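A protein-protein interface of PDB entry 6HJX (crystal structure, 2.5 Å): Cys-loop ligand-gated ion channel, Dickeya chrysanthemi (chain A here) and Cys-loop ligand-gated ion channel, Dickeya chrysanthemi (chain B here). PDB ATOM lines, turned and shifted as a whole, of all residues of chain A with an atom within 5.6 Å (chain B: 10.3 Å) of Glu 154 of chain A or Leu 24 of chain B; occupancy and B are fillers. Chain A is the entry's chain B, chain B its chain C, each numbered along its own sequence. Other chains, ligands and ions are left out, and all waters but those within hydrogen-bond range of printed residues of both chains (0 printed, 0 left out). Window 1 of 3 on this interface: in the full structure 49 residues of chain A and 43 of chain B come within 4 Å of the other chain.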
ATOM      1  N   GLU A 150     -24.741  19.155  21.900  1.00  0.00           N
ATOM      2  CA  GLU A 150     -23.613  19.216  22.821  1.00  0.00           C
ATOM      3  C   GLU A 150     -23.747  18.270  24.012  1.00  0.00           C
ATOM      4  O   GLU A 150     -22.899  18.315  24.910  1.00  0.00           O
ATOM      5  CB  GLU A 150     -23.438  20.652  23.330  1.00  0.00           C
ATOM      6  CG  GLU A 150     -24.633  21.193  24.107  1.00  0.00           C
ATOM      7  CD  GLU A 150     -24.405  22.601  24.623  1.00  0.00           C
ATOM      8  OE1 GLU A 150     -23.622  23.346  23.996  1.00  0.00           O
ATOM      9  OE2 GLU A 150     -25.005  22.962  25.658  1.00  0.00           O
ATOM     10  N   ILE A 152     -23.212  15.104  24.324  1.00  0.00           N
ATOM     11  CA  ILE A 152     -22.128  14.131  24.421  1.00  0.00           C
ATOM     12  C   ILE A 152     -20.776  14.834  24.470  1.00  0.00           C
ATOM     13  O   ILE A 152     -19.725  14.181  24.434  1.00  0.00           O
ATOM     14  CB  ILE A 152     -22.166  13.133  23.246  1.00  0.00           C
ATOM     15  CG1 ILE A 152     -22.040  13.869  21.905  1.00  0.00           C
ATOM     16  CG2 ILE A 152     -23.443  12.314  23.295  1.00  0.00           C
ATOM     17  CD1 ILE A 152     -21.760  12.954  20.723  1.00  0.00           C
ATOM     18  N   ASP A 153     -20.786  16.161  24.547  1.00  0.00           N
ATOM     19  CA  ASP A 153     -19.555  16.936  24.495  1.00  0.00           C
ATOM     20  C   ASP A 153     -19.032  17.224  25.894  1.00  0.00           C
ATOM     21  O   ASP A 153     -19.795  17.567  26.803  1.00  0.00           O
ATOM     22  CB  ASP A 153     -19.778  18.247  23.740  1.00  0.00           C
ATOM     23  CG  ASP A 153     -19.836  18.050  22.236  1.00  0.00           C
ATOM     24  OD1 ASP A 153     -19.198  17.097  21.733  1.00  0.00           O
ATOM     25  OD2 ASP A 153     -20.515  18.850  21.556  1.00  0.00           O
ATOM     26  N   GLU A 154     -17.714  17.080  26.057  1.00  0.00           N
ATOM     27  CA  GLU A 154     -17.085  17.374  27.339  1.00  0.00           C
ATOM     28  C   GLU A 154     -17.258  18.841  27.710  1.00  0.00           C
ATOM     29  O   GLU A 154     -17.464  19.171  28.883  1.00  0.00           O
ATOM     30  CB  GLU A 154     -15.604  17.006  27.286  1.00  0.00           C
ATOM     31  CG  GLU A 154     -14.895  17.089  28.625  1.00  0.00           C
ATOM     32  CD  GLU A 154     -13.507  16.496  28.574  1.00  0.00           C
ATOM     33  OE1 GLU A 154     -13.019  16.223  27.458  1.00  0.00           O
ATOM     34  OE2 GLU A 154     -12.904  16.295  29.649  1.00  0.00           O
ATOM     35  N   TRP A 155     -17.188  19.731  26.723  1.00  0.00           N
ATOM     36  CA  TRP A 155     -17.316  21.165  26.943  1.00  0.00           C
ATOM     37  C   TRP A 155     -18.481  21.712  26.131  1.00  0.00           C
ATOM     38  O   TRP A 155     -18.745  21.251  25.015  1.00  0.00           O
ATOM     39  CB  TRP A 155     -16.024  21.894  26.561  1.00  0.00           C
ATOM     40  CG  TRP A 155     -14.861  21.502  27.404  1.00  0.00           C
ATOM     41  CD1 TRP A 155     -13.959  20.511  27.149  1.00  0.00           C
ATOM     42  CD2 TRP A 155     -14.471  22.089  28.649  1.00  0.00           C
ATOM     43  NE1 TRP A 155     -13.031  20.446  28.158  1.00  0.00           N
ATOM     44  CE2 TRP A 155     -13.322  21.406  29.090  1.00  0.00           C
ATOM     45  CE3 TRP A 155     -14.981  23.127  29.432  1.00  0.00           C
ATOM     46  CZ2 TRP A 155     -12.677  21.727  30.279  1.00  0.00           C
ATOM     47  CZ3 TRP A 155     -14.339  23.445  30.610  1.00  0.00           C
ATOM     48  CH2 TRP A 155     -13.200  22.748  31.024  1.00  0.00           C
ATOM     49  N   TRP A 156     -19.175  22.696  26.699  1.00  0.00           N
ATOM     50  CA  TRP A 156     -20.294  23.365  26.043  1.00  0.00           C
ATOM     51  C   TRP A 156     -19.868  24.787  25.698  1.00  0.00           C
ATOM     52  O   TRP A 156     -19.657  25.612  26.592  1.00  0.00           O
ATOM     53  CB  TRP A 156     -21.530  23.372  26.941  1.00  0.00           C
ATOM     54  CG  TRP A 156     -22.058  22.001  27.266  1.00  0.00           C
ATOM     55  CD1 TRP A 156     -21.771  20.834  26.618  1.00  0.00           C
ATOM     56  CD2 TRP A 156     -22.962  21.660  28.324  1.00  0.00           C
ATOM     57  NE1 TRP A 156     -22.442  19.790  27.206  1.00  0.00           N
ATOM     58  CE2 TRP A 156     -23.179  20.270  28.256  1.00  0.00           C
ATOM     59  CE3 TRP A 156     -23.606  22.396  29.323  1.00  0.00           C
ATOM     60  CZ2 TRP A 156     -24.016  19.602  29.147  1.00  0.00           C
ATOM     61  CZ3 TRP A 156     -24.437  21.730  30.207  1.00  0.00           C
ATOM     62  CH2 TRP A 156     -24.634  20.347  30.113  1.00  0.00           C
ATOM     63  N   VAL A 193     -18.176  25.987  28.963  1.00  0.00           N
ATOM     64  CA  VAL A 193     -18.531  25.484  30.282  1.00  0.00           C
ATOM     65  C   VAL A 193     -18.401  23.970  30.248  1.00  0.00           C
ATOM     66  O   VAL A 193     -18.762  23.331  29.253  1.00  0.00           O
ATOM     67  CB  VAL A 193     -19.960  25.897  30.690  1.00  0.00           C
ATOM     68  CG1 VAL A 193     -20.310  25.327  32.058  1.00  0.00           C
ATOM     69  CG2 VAL A 193     -20.100  27.413  30.692  1.00  0.00           C
ATOM     70  N   ARG A 194     -17.883  23.397  31.329  1.00  0.00           N
ATOM     71  CA  ARG A 194     -17.738  21.952  31.400  1.00  0.00           C
ATOM     72  C   ARG A 194     -19.109  21.293  31.490  1.00  0.00           C
ATOM     73  O   ARG A 194     -20.017  21.800  32.156  1.00  0.00           O
ATOM     74  CB  ARG A 194     -16.886  21.559  32.607  1.00  0.00           C
ATOM     75  CG  ARG A 194     -16.557  20.075  32.675  1.00  0.00           C
ATOM     76  CD  ARG A 194     -15.832  19.723  33.965  1.00  0.00           C
ATOM     77  NE  ARG A 194     -14.648  20.556  34.168  1.00  0.00           N
ATOM     78  CZ  ARG A 194     -13.464  20.326  33.608  1.00  0.00           C
ATOM     79  NH1 ARG A 194     -13.291  19.285  32.802  1.00  0.00           N
ATOM     80  NH2 ARG A 194     -12.448  21.143  33.852  1.00  0.00           N
ATOM     81  N   ASN A 195     -19.260  20.169  30.798  1.00  0.00           N
ATOM     82  CA  ASN A 195     -20.449  19.338  30.942  1.00  0.00           C
ATOM     83  C   ASN A 195     -20.346  18.562  32.253  1.00  0.00           C
ATOM     84  O   ASN A 195     -19.578  17.596  32.334  1.00  0.00           O
ATOM     85  CB  ASN A 195     -20.586  18.376  29.760  1.00  0.00           C
ATOM     86  CG  ASN A 195     -21.721  17.382  29.945  1.00  0.00           C
ATOM     87  OD1 ASN A 195     -22.652  17.622  30.715  1.00  0.00           O
ATOM     88  ND2 ASN A 195     -21.645  16.255  29.241  1.00  0.00           N
ATOM     89  N   TYR A 199     -19.961  13.924  36.235  1.00  0.00           N
ATOM     90  CA  TYR A 199     -19.465  14.122  37.591  1.00  0.00           C
ATOM     91  C   TYR A 199     -20.589  14.271  38.609  1.00  0.00           C
ATOM     92  O   TYR A 199     -20.379  13.981  39.792  1.00  0.00           O
ATOM     93  CB  TYR A 199     -18.544  15.347  37.629  1.00  0.00           C
ATOM     94  CG  TYR A 199     -17.415  15.257  36.622  1.00  0.00           C
ATOM     95  CD1 TYR A 199     -16.291  14.483  36.878  1.00  0.00           C
ATOM     96  CD2 TYR A 199     -17.484  15.929  35.406  1.00  0.00           C
ATOM     97  CE1 TYR A 199     -15.268  14.386  35.963  1.00  0.00           C
ATOM     98  CE2 TYR A 199     -16.463  15.837  34.482  1.00  0.00           C
ATOM     99  CZ  TYR A 199     -15.358  15.064  34.767  1.00  0.00           C
ATOM    100  OH  TYR A 199     -14.336  14.966  33.853  1.00  0.00           O
ATOM    101  N   GLY B  20      -6.691   1.506  18.280  1.00  0.00           N
ATOM    102  CA  GLY B  20      -6.293   2.631  19.110  1.00  0.00           C
ATOM    103  C   GLY B  20      -7.375   3.665  19.328  1.00  0.00           C
ATOM    104  O   GLY B  20      -7.078   4.865  19.379  1.00  0.00           O
ATOM    105  N   VAL B  21      -8.629   3.228  19.457  1.00  0.00           N
ATOM    106  CA  VAL B  21      -9.703   4.159  19.780  1.00  0.00           C
ATOM    107  C   VAL B  21      -9.356   4.892  21.066  1.00  0.00           C
ATOM    108  O   VAL B  21      -8.981   4.275  22.070  1.00  0.00           O
ATOM    109  CB  VAL B  21     -11.042   3.418  19.909  1.00  0.00           C
ATOM    110  CG1 VAL B  21     -12.134   4.362  20.411  1.00  0.00           C
ATOM    111  CG2 VAL B  21     -11.447   2.809  18.576  1.00  0.00           C
ATOM    112  N   ASN B  22      -9.459   6.217  21.031  1.00  0.00           N
ATOM    113  CA  ASN B  22      -9.340   7.060  22.218  1.00  0.00           C
ATOM    114  C   ASN B  22     -10.706   7.691  22.446  1.00  0.00           C
ATOM    115  O   ASN B  22     -11.140   8.543  21.664  1.00  0.00           O
ATOM    116  CB  ASN B  22      -8.253   8.116  22.041  1.00  0.00           C
ATOM    117  CG  ASN B  22      -8.071   8.981  23.272  1.00  0.00           C
ATOM    118  OD1 ASN B  22      -9.033   9.306  23.968  1.00  0.00           O
ATOM    119  ND2 ASN B  22      -6.828   9.364  23.545  1.00  0.00           N
ATOM    120  N   THR B  23     -11.385   7.269  23.514  1.00  0.00           N
ATOM    121  CA  THR B  23     -12.790   7.623  23.677  1.00  0.00           C
ATOM    122  C   THR B  23     -12.966   9.096  24.035  1.00  0.00           C
ATOM    123  O   THR B  23     -13.833   9.774  23.472  1.00  0.00           O
ATOM    124  CB  THR B  23     -13.434   6.727  24.736  1.00  0.00           C
ATOM    125  OG1 THR B  23     -12.682   6.793  25.953  1.00  0.00           O
ATOM    126  CG2 THR B  23     -13.484   5.289  24.249  1.00  0.00           C
ATOM    127  N   LEU B  24     -12.159   9.616  24.962  1.00  0.00           N
ATOM    128  CA  LEU B  24     -12.327  11.005  25.374  1.00  0.00           C
ATOM    129  C   LEU B  24     -12.055  11.960  24.217  1.00  0.00           C
ATOM    130  O   LEU B  24     -12.772  12.952  24.038  1.00  0.00           O
ATOM    131  CB  LEU B  24     -11.409  11.328  26.549  1.00  0.00           C
ATOM    132  CG  LEU B  24     -11.800  12.606  27.297  1.00  0.00           C
ATOM    133  CD1 LEU B  24     -12.843  12.284  28.356  1.00  0.00           C
ATOM    134  CD2 LEU B  24     -10.588  13.298  27.909  1.00  0.00           C
ATOM    135  N   GLU B  25     -11.021  11.682  23.426  1.00  0.00           N
ATOM    136  CA  GLU B  25     -10.692  12.519  22.279  1.00  0.00           C
ATOM    137  C   GLU B  25     -11.512  12.175  21.046  1.00  0.00           C
ATOM    138  O   GLU B  25     -11.469  12.926  20.067  1.00  0.00           O
ATOM    139  CB  GLU B  25      -9.202  12.395  21.946  1.00  0.00           C
ATOM    140  CG  GLU B  25      -8.273  12.895  23.045  1.00  0.00           C
ATOM    141  CD  GLU B  25      -6.805  12.804  22.661  1.00  0.00           C
ATOM    142  OE1 GLU B  25      -6.499  12.192  21.613  1.00  0.00           O
ATOM    143  OE2 GLU B  25      -5.960  13.347  23.406  1.00  0.00           O
ATOM    144  N   GLN B  26     -12.253  11.070  21.073  1.00  0.00           N
ATOM    145  CA  GLN B  26     -13.036  10.621  19.925  1.00  0.00           C
ATOM    146  C   GLN B  26     -12.152  10.505  18.686  1.00  0.00           C
ATOM    147  O   GLN B  26     -12.455  11.040  17.619  1.00  0.00           O
ATOM    148  CB  GLN B  26     -14.224  11.554  19.681  1.00  0.00           C
ATOM    149  CG  GLN B  26     -15.148  11.694  20.893  1.00  0.00           C
ATOM    150  CD  GLN B  26     -16.404  12.498  20.604  1.00  0.00           C
ATOM    151  OE1 GLN B  26     -17.029  12.342  19.557  1.00  0.00           O
ATOM    152  NE2 GLN B  26     -16.782  13.360  21.541  1.00  0.00           N
ATOM    153  N   THR B  27     -11.038   9.794  18.840  1.00  0.00           N
ATOM    154  CA  THR B  27     -10.116   9.547  17.745  1.00  0.00           C
ATOM    155  C   THR B  27      -9.866   8.051  17.604  1.00  0.00           C
ATOM    156  O   THR B  27     -10.255   7.241  18.451  1.00  0.00           O
ATOM    157  CB  THR B  27      -8.781  10.275  17.950  1.00  0.00           C
ATOM    158  OG1 THR B  27      -8.154   9.798  19.147  1.00  0.00           O
ATOM    159  CG2 THR B  27      -8.990  11.784  18.048  1.00  0.00           C
ATOM    160  N   TYR B  28      -9.203   7.698  16.506  1.00  0.00           N
ATOM    161  CA  TYR B  28      -8.834   6.321  16.212  1.00  0.00           C
ATOM    162  C   TYR B  28      -7.709   6.355  15.189  1.00  0.00           C
ATOM    163  O   TYR B  28      -7.522   7.349  14.483  1.00  0.00           O
ATOM    164  CB  TYR B  28     -10.030   5.511  15.696  1.00  0.00           C
ATOM    165  CG  TYR B  28     -10.770   6.195  14.575  1.00  0.00           C
ATOM    166  CD1 TYR B  28     -11.787   7.095  14.844  1.00  0.00           C
ATOM    167  CD2 TYR B  28     -10.443   5.956  13.247  1.00  0.00           C
ATOM    168  CE1 TYR B  28     -12.462   7.735  13.828  1.00  0.00           C
ATOM    169  CE2 TYR B  28     -11.117   6.593  12.220  1.00  0.00           C
ATOM    170  CZ  TYR B  28     -12.123   7.487  12.519  1.00  0.00           C
ATOM    171  OH  TYR B  28     -12.805   8.133  11.511  1.00  0.00           O
ATOM    172  N   PHE B 105      -7.471   9.763  13.375  1.00  0.00           N
ATOM    173  CA  PHE B 105      -8.614  10.415  12.757  1.00  0.00           C
ATOM    174  C   PHE B 105      -9.700  10.649  13.794  1.00  0.00           C
ATOM    175  O   PHE B 105      -9.901   9.828  14.691  1.00  0.00           O
ATOM    176  CB  PHE B 105      -9.153   9.576  11.592  1.00  0.00           C
ATOM    177  CG  PHE B 105      -8.173   9.417  10.462  1.00  0.00           C
ATOM    178  CD1 PHE B 105      -7.149   8.485  10.543  1.00  0.00           C
ATOM    179  CD2 PHE B 105      -8.271  10.204   9.325  1.00  0.00           C
ATOM    180  CE1 PHE B 105      -6.242   8.341   9.510  1.00  0.00           C
ATOM    181  CE2 PHE B 105      -7.365  10.064   8.287  1.00  0.00           C
ATOM    182  CZ  PHE B 105      -6.351   9.134   8.380  1.00  0.00           C
ATOM    183  N   SER B 106     -10.391  11.777  13.666  1.00  0.00           N
ATOM    184  CA  SER B 106     -11.454  12.156  14.583  1.00  0.00           C
ATOM    185  C   SER B 106     -12.814  11.941  13.929  1.00  0.00           C
ATOM    186  O   SER B 106     -12.948  11.926  12.704  1.00  0.00           O
ATOM    187  CB  SER B 106     -11.309  13.619  15.011  1.00  0.00           C
ATOM    188  OG  SER B 106     -11.885  14.489  14.051  1.00  0.00           O
ATOM    189  N   ASN B 107     -13.827  11.755  14.766  1.00  0.00           N
ATOM    190  CA  ASN B 107     -15.198  11.630  14.290  1.00  0.00           C
ATOM    191  C   ASN B 107     -16.117  11.727  15.498  1.00  0.00           C
ATOM    192  O   ASN B 107     -15.675  11.672  16.648  1.00  0.00           O
ATOM    193  CB  ASN B 107     -15.429  10.318  13.536  1.00  0.00           C
ATOM    194  CG  ASN B 107     -15.419   9.109  14.450  1.00  0.00           C
ATOM    195  OD1 ASN B 107     -14.661   9.059  15.419  1.00  0.00           O
ATOM    196  ND2 ASN B 107     -16.260   8.126  14.148  1.00  0.00           N
ATOM    197  N   ASP B 108     -17.406  11.876  15.216  1.00  0.00           N
ATOM    198  CA  ASP B 108     -18.421  11.959  16.259  1.00  0.00           C
ATOM    199  C   ASP B 108     -18.724  10.547  16.738  1.00  0.00           C
ATOM    200  O   ASP B 108     -19.317   9.749  16.004  1.00  0.00           O
ATOM    201  CB  ASP B 108     -19.673  12.652  15.737  1.00  0.00           C
ATOM    202  CG  ASP B 108     -19.406  14.073  15.289  1.00  0.00           C
ATOM    203  OD1 ASP B 108     -18.664  14.788  15.993  1.00  0.00           O
ATOM    204  OD2 ASP B 108     -19.932  14.475  14.233  1.00  0.00           O
ATOM    205  N   MET B 109     -18.304  10.228  17.960  1.00  0.00           N
ATOM    206  CA  MET B 109     -18.473   8.900  18.529  1.00  0.00           C
ATOM    207  C   MET B 109     -19.304   9.005  19.798  1.00  0.00           C
ATOM    208  O   MET B 109     -19.057   9.878  20.635  1.00  0.00           O
ATOM    209  CB  MET B 109     -17.117   8.256  18.821  1.00  0.00           C
ATOM    210  CG  MET B 109     -16.217   8.198  17.602  1.00  0.00           C
ATOM    211  SD  MET B 109     -14.686   7.278  17.852  1.00  0.00           S
ATOM    212  CE  MET B 109     -15.300   5.595  17.826  1.00  0.00           C
ATOM    213  N   ASP B 110     -20.283   8.114  19.930  1.00  0.00           N
ATOM    214  CA  ASP B 110     -21.227   8.114  21.043  1.00  0.00           C
ATOM    215  C   ASP B 110     -21.093   6.783  21.769  1.00  0.00           C
ATOM    216  O   ASP B 110     -21.447   5.734  21.221  1.00  0.00           O
ATOM    217  CB  ASP B 110     -22.653   8.333  20.536  1.00  0.00           C
ATOM    218  CG  ASP B 110     -23.644   8.560  21.654  1.00  0.00           C
ATOM    219  OD1 ASP B 110     -23.274   8.383  22.833  1.00  0.00           O
ATOM    220  OD2 ASP B 110     -24.799   8.925  21.350  1.00  0.00           O
ATOM    221  N   PHE B 111     -20.581   6.825  23.001  1.00  0.00           N
ATOM    222  CA  PHE B 111     -20.309   5.622  23.777  1.00  0.00           C
ATOM    223  C   PHE B 111     -21.305   5.424  24.917  1.00  0.00           C
ATOM    224  O   PHE B 111     -21.031   4.657  25.846  1.00  0.00           O
ATOM    225  CB  PHE B 111     -18.883   5.665  24.327  1.00  0.00           C
ATOM    226  CG  PHE B 111     -17.826   5.755  23.263  1.00  0.00           C
ATOM    227  CD1 PHE B 111     -17.520   4.655  22.478  1.00  0.00           C
ATOM    228  CD2 PHE B 111     -17.133   6.937  23.052  1.00  0.00           C
ATOM    229  CE1 PHE B 111     -16.548   4.732  21.498  1.00  0.00           C
ATOM    230  CE2 PHE B 111     -16.157   7.020  22.073  1.00  0.00           C
ATOM    231  CZ  PHE B 111     -15.865   5.915  21.295  1.00  0.00           C
ATOM    232  N   ARG B 194     -19.071  -3.078  18.769  1.00  0.00           N
ATOM    233  CA  ARG B 194     -18.143  -3.536  19.790  1.00  0.00           C
ATOM    234  C   ARG B 194     -18.438  -4.980  20.183  1.00  0.00           C
ATOM    235  O   ARG B 194     -19.567  -5.463  20.062  1.00  0.00           O
ATOM    236  CB  ARG B 194     -18.219  -2.636  21.025  1.00  0.00           C
ATOM    237  CG  ARG B 194     -17.168  -2.941  22.085  1.00  0.00           C
ATOM    238  CD  ARG B 194     -17.363  -2.092  23.330  1.00  0.00           C
ATOM    239  NE  ARG B 194     -17.345  -0.663  23.028  1.00  0.00           N
ATOM    240  CZ  ARG B 194     -16.240   0.065  22.898  1.00  0.00           C
ATOM    241  NH1 ARG B 194     -15.046  -0.492  23.039  1.00  0.00           N
ATOM    242  NH2 ARG B 194     -16.331   1.358  22.622  1.00  0.00           N
ATOM    243  N   LEU B 248     -12.151   0.554  32.284  1.00  0.00           N
ATOM    244  CA  LEU B 248     -13.074   1.036  31.273  1.00  0.00           C
ATOM    245  C   LEU B 248     -12.654   2.422  30.787  1.00  0.00           C
ATOM    246  O   LEU B 248     -11.938   3.147  31.480  1.00  0.00           O
ATOM    247  CB  LEU B 248     -14.495   1.067  31.832  1.00  0.00           C
ATOM    248  CG  LEU B 248     -15.062  -0.301  32.228  1.00  0.00           C
ATOM    249  CD1 LEU B 248     -16.438  -0.157  32.855  1.00  0.00           C
ATOM    250  CD2 LEU B 248     -15.122  -1.247  31.031  1.00  0.00           C
ATOM    251  N   PRO B 249     -13.088   2.811  29.589  1.00  0.00           N
ATOM    252  CA  PRO B 249     -12.603   4.065  29.007  1.00  0.00           C
ATOM    253  C   PRO B 249     -13.214   5.290  29.666  1.00  0.00           C
ATOM    254  O   PRO B 249     -14.340   5.264  30.172  1.00  0.00           O
ATOM    255  CB  PRO B 249     -13.034   3.957  27.540  1.00  0.00           C
ATOM    256  CG  PRO B 249     -14.253   3.119  27.581  1.00  0.00           C
ATOM    257  CD  PRO B 249     -14.037   2.125  28.694  1.00  0.00           C
ATOM    258  N   ARG B 250     -12.447   6.376  29.644  1.00  0.00           N
ATOM    259  CA  ARG B 250     -12.895   7.647  30.190  1.00  0.00           C
ATOM    260  C   ARG B 250     -13.836   8.340  29.213  1.00  0.00           C
ATOM    261  O   ARG B 250     -13.620   8.320  27.998  1.00  0.00           O
ATOM    262  CB  ARG B 250     -11.697   8.545  30.493  1.00  0.00           C
ATOM    263  CG  ARG B 250     -10.878   8.089  31.690  1.00  0.00           C
ATOM    264  CD  ARG B 250     -11.536   8.478  33.010  1.00  0.00           C
ATOM    265  NE  ARG B 250     -11.484   9.921  33.245  1.00  0.00           N
ATOM    266  CZ  ARG B 250     -12.470  10.775  32.976  1.00  0.00           C
ATOM    267  NH1 ARG B 250     -13.615  10.350  32.457  1.00  0.00           N
ATOM    268  NH2 ARG B 250     -12.307  12.067  33.232  1.00  0.00           N
ATOM    269  N   LEU B 251     -14.882   8.956  29.754  1.00  0.00           N
ATOM    270  CA  LEU B 251     -15.914   9.594  28.952  1.00  0.00           C
ATOM    271  C   LEU B 251     -16.436  10.806  29.707  1.00  0.00           C
ATOM    272  O   LEU B 251     -16.256  10.906  30.926  1.00  0.00           O
ATOM    273  CB  LEU B 251     -17.069   8.631  28.652  1.00  0.00           C
ATOM    274  CG  LEU B 251     -16.735   7.345  27.899  1.00  0.00           C
ATOM    275  CD1 LEU B 251     -17.913   6.389  27.952  1.00  0.00           C
ATOM    276  CD2 LEU B 251     -16.362   7.651  26.460  1.00  0.00           C
ATOM    277  N   PRO B 252     -17.086  11.738  29.016  1.00  0.00           N
ATOM    278  CA  PRO B 252     -17.774  12.846  29.695  1.00  0.00           C
ATOM    279  C   PRO B 252     -19.224  12.564  30.068  1.00  0.00           C
ATOM    280  O   PRO B 252     -19.939  13.504  30.424  1.00  0.00           O
ATOM    281  CB  PRO B 252     -17.700  13.963  28.647  1.00  0.00           C
ATOM    282  CG  PRO B 252     -17.774  13.240  27.345  1.00  0.00           C
ATOM    283  CD  PRO B 252     -17.110  11.897  27.549  1.00  0.00           C
ATOM    284  N   TYR B 253     -19.668  11.310  29.994  1.00  0.00           N
ATOM    285  CA  TYR B 253     -21.033  10.942  30.342  1.00  0.00           C
ATOM    286  C   TYR B 253     -21.020   9.542  30.941  1.00  0.00           C
ATOM    287  O   TYR B 253     -19.999   8.852  30.934  1.00  0.00           O
ATOM    288  CB  TYR B 253     -21.957  11.006  29.121  1.00  0.00           C
ATOM    289  CG  TYR B 253     -21.326  10.477  27.854  1.00  0.00           C
ATOM    290  CD1 TYR B 253     -21.276   9.114  27.593  1.00  0.00           C
ATOM    291  CD2 TYR B 253     -20.782  11.343  26.915  1.00  0.00           C
ATOM    292  CE1 TYR B 253     -20.700   8.630  26.433  1.00  0.00           C
ATOM    293  CE2 TYR B 253     -20.205  10.870  25.755  1.00  0.00           C
ATOM    294  CZ  TYR B 253     -20.166   9.513  25.517  1.00  0.00           C
ATOM    295  OH  TYR B 253     -19.591   9.041  24.361  1.00  0.00           O
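ND2 of Asn 195 of chain A lies within hydrogen-bond range of O of Pro 252 of chain B (3.4 Å).
OH of Tyr 253 of chain B lies within hydrogen-bond range of N of Phe 111 of chain B (2.8 Å). The backbone NH of Leu 24 of chain B sits at hydrogen-bond distance from the side-chain amide oxygen of Asn 22 of chain B (3.3 Å). The backbone NH (N) of Asn 195 of chain A lies within hydrogen-bond range of the backbone carbonyl oxygen (O) of Glu 154 of chain A (2.8 Å). The backbone carbonyl oxygen of Asp 153 of chain A sits close to the side-chain amide nitrogen of Asn 195 of chain A. OG1 of Thr 23 of chain B lies within hydrogen-bond range of O of Arg 250 of chain B (2.7 Å).
Asp 110 of chain B touches Ile 152 of chain A (OD1 to CG2, 3.96 Å). CG of Pro 252 of chain B touches O of Ile 152 of chain A, 3.6 Å away. Ile 152 of chain A touches Tyr 253 of chain B (O to CE2, 3.6 Å). Glu 154 of chain A touches Leu 24 of chain B. Pro 252 of chain B touches Glu 154 of chain A. Tyr 199 of chain A touches Arg 250 of chain B (OH to NH2, 3.6 Å).
Of chain B, only Leu 24 (3.8 Å) and Pro 252 (3.7 Å) come within 4 Å of Glu 154 of chain A. Of chain A, only Glu 154 comes within 4 Å of Leu 24 of chain B. Trp 155 of chain A touches none of the printed residues of chain B. Of chain B, only Pro 252 comes within 4 Å of Asn 195 of chain A. Printed residues of chain A within 4 Å of Arg 250 of chain B: Tyr 199 (3.6 Å). Of the printed residues of chain B, Tyr 199 of chain A touches Arg 250. Met 109 of chain B touches none of the printed residues of chain A. The nearest printed residue of chain A that does not touch Leu 24 of chain B is Tyr 199 of chain A (6.3 Å). The nearest printed residue of chain B that does not touch Ile 152 of chain A is Met 109 of chain B (4.1 Å).
Of the 23 printed residues of chain B, 5 touch a printed residue of chain A. Hydrophobic or aromatic side chains of chain B that line the printed part of chain A: Leu 24, Pro 252 and Tyr 253. Along chain B the printed residues that touch a printed residue of chain A span positions 24 to 253. Of the 10 printed residues of chain A, 4 touch a printed residue of chain B. Printed residues of chain A that touch a printed residue of chain B: Ile 152, Glu 154, Asn 195 and Tyr 199. Among the printed residues, 7 pairs touch across the chains. Among the printed residues, no Asp or Glu carboxylate lies within 4 Å of a Lys or Arg side-chain nitrogen of the other chain.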
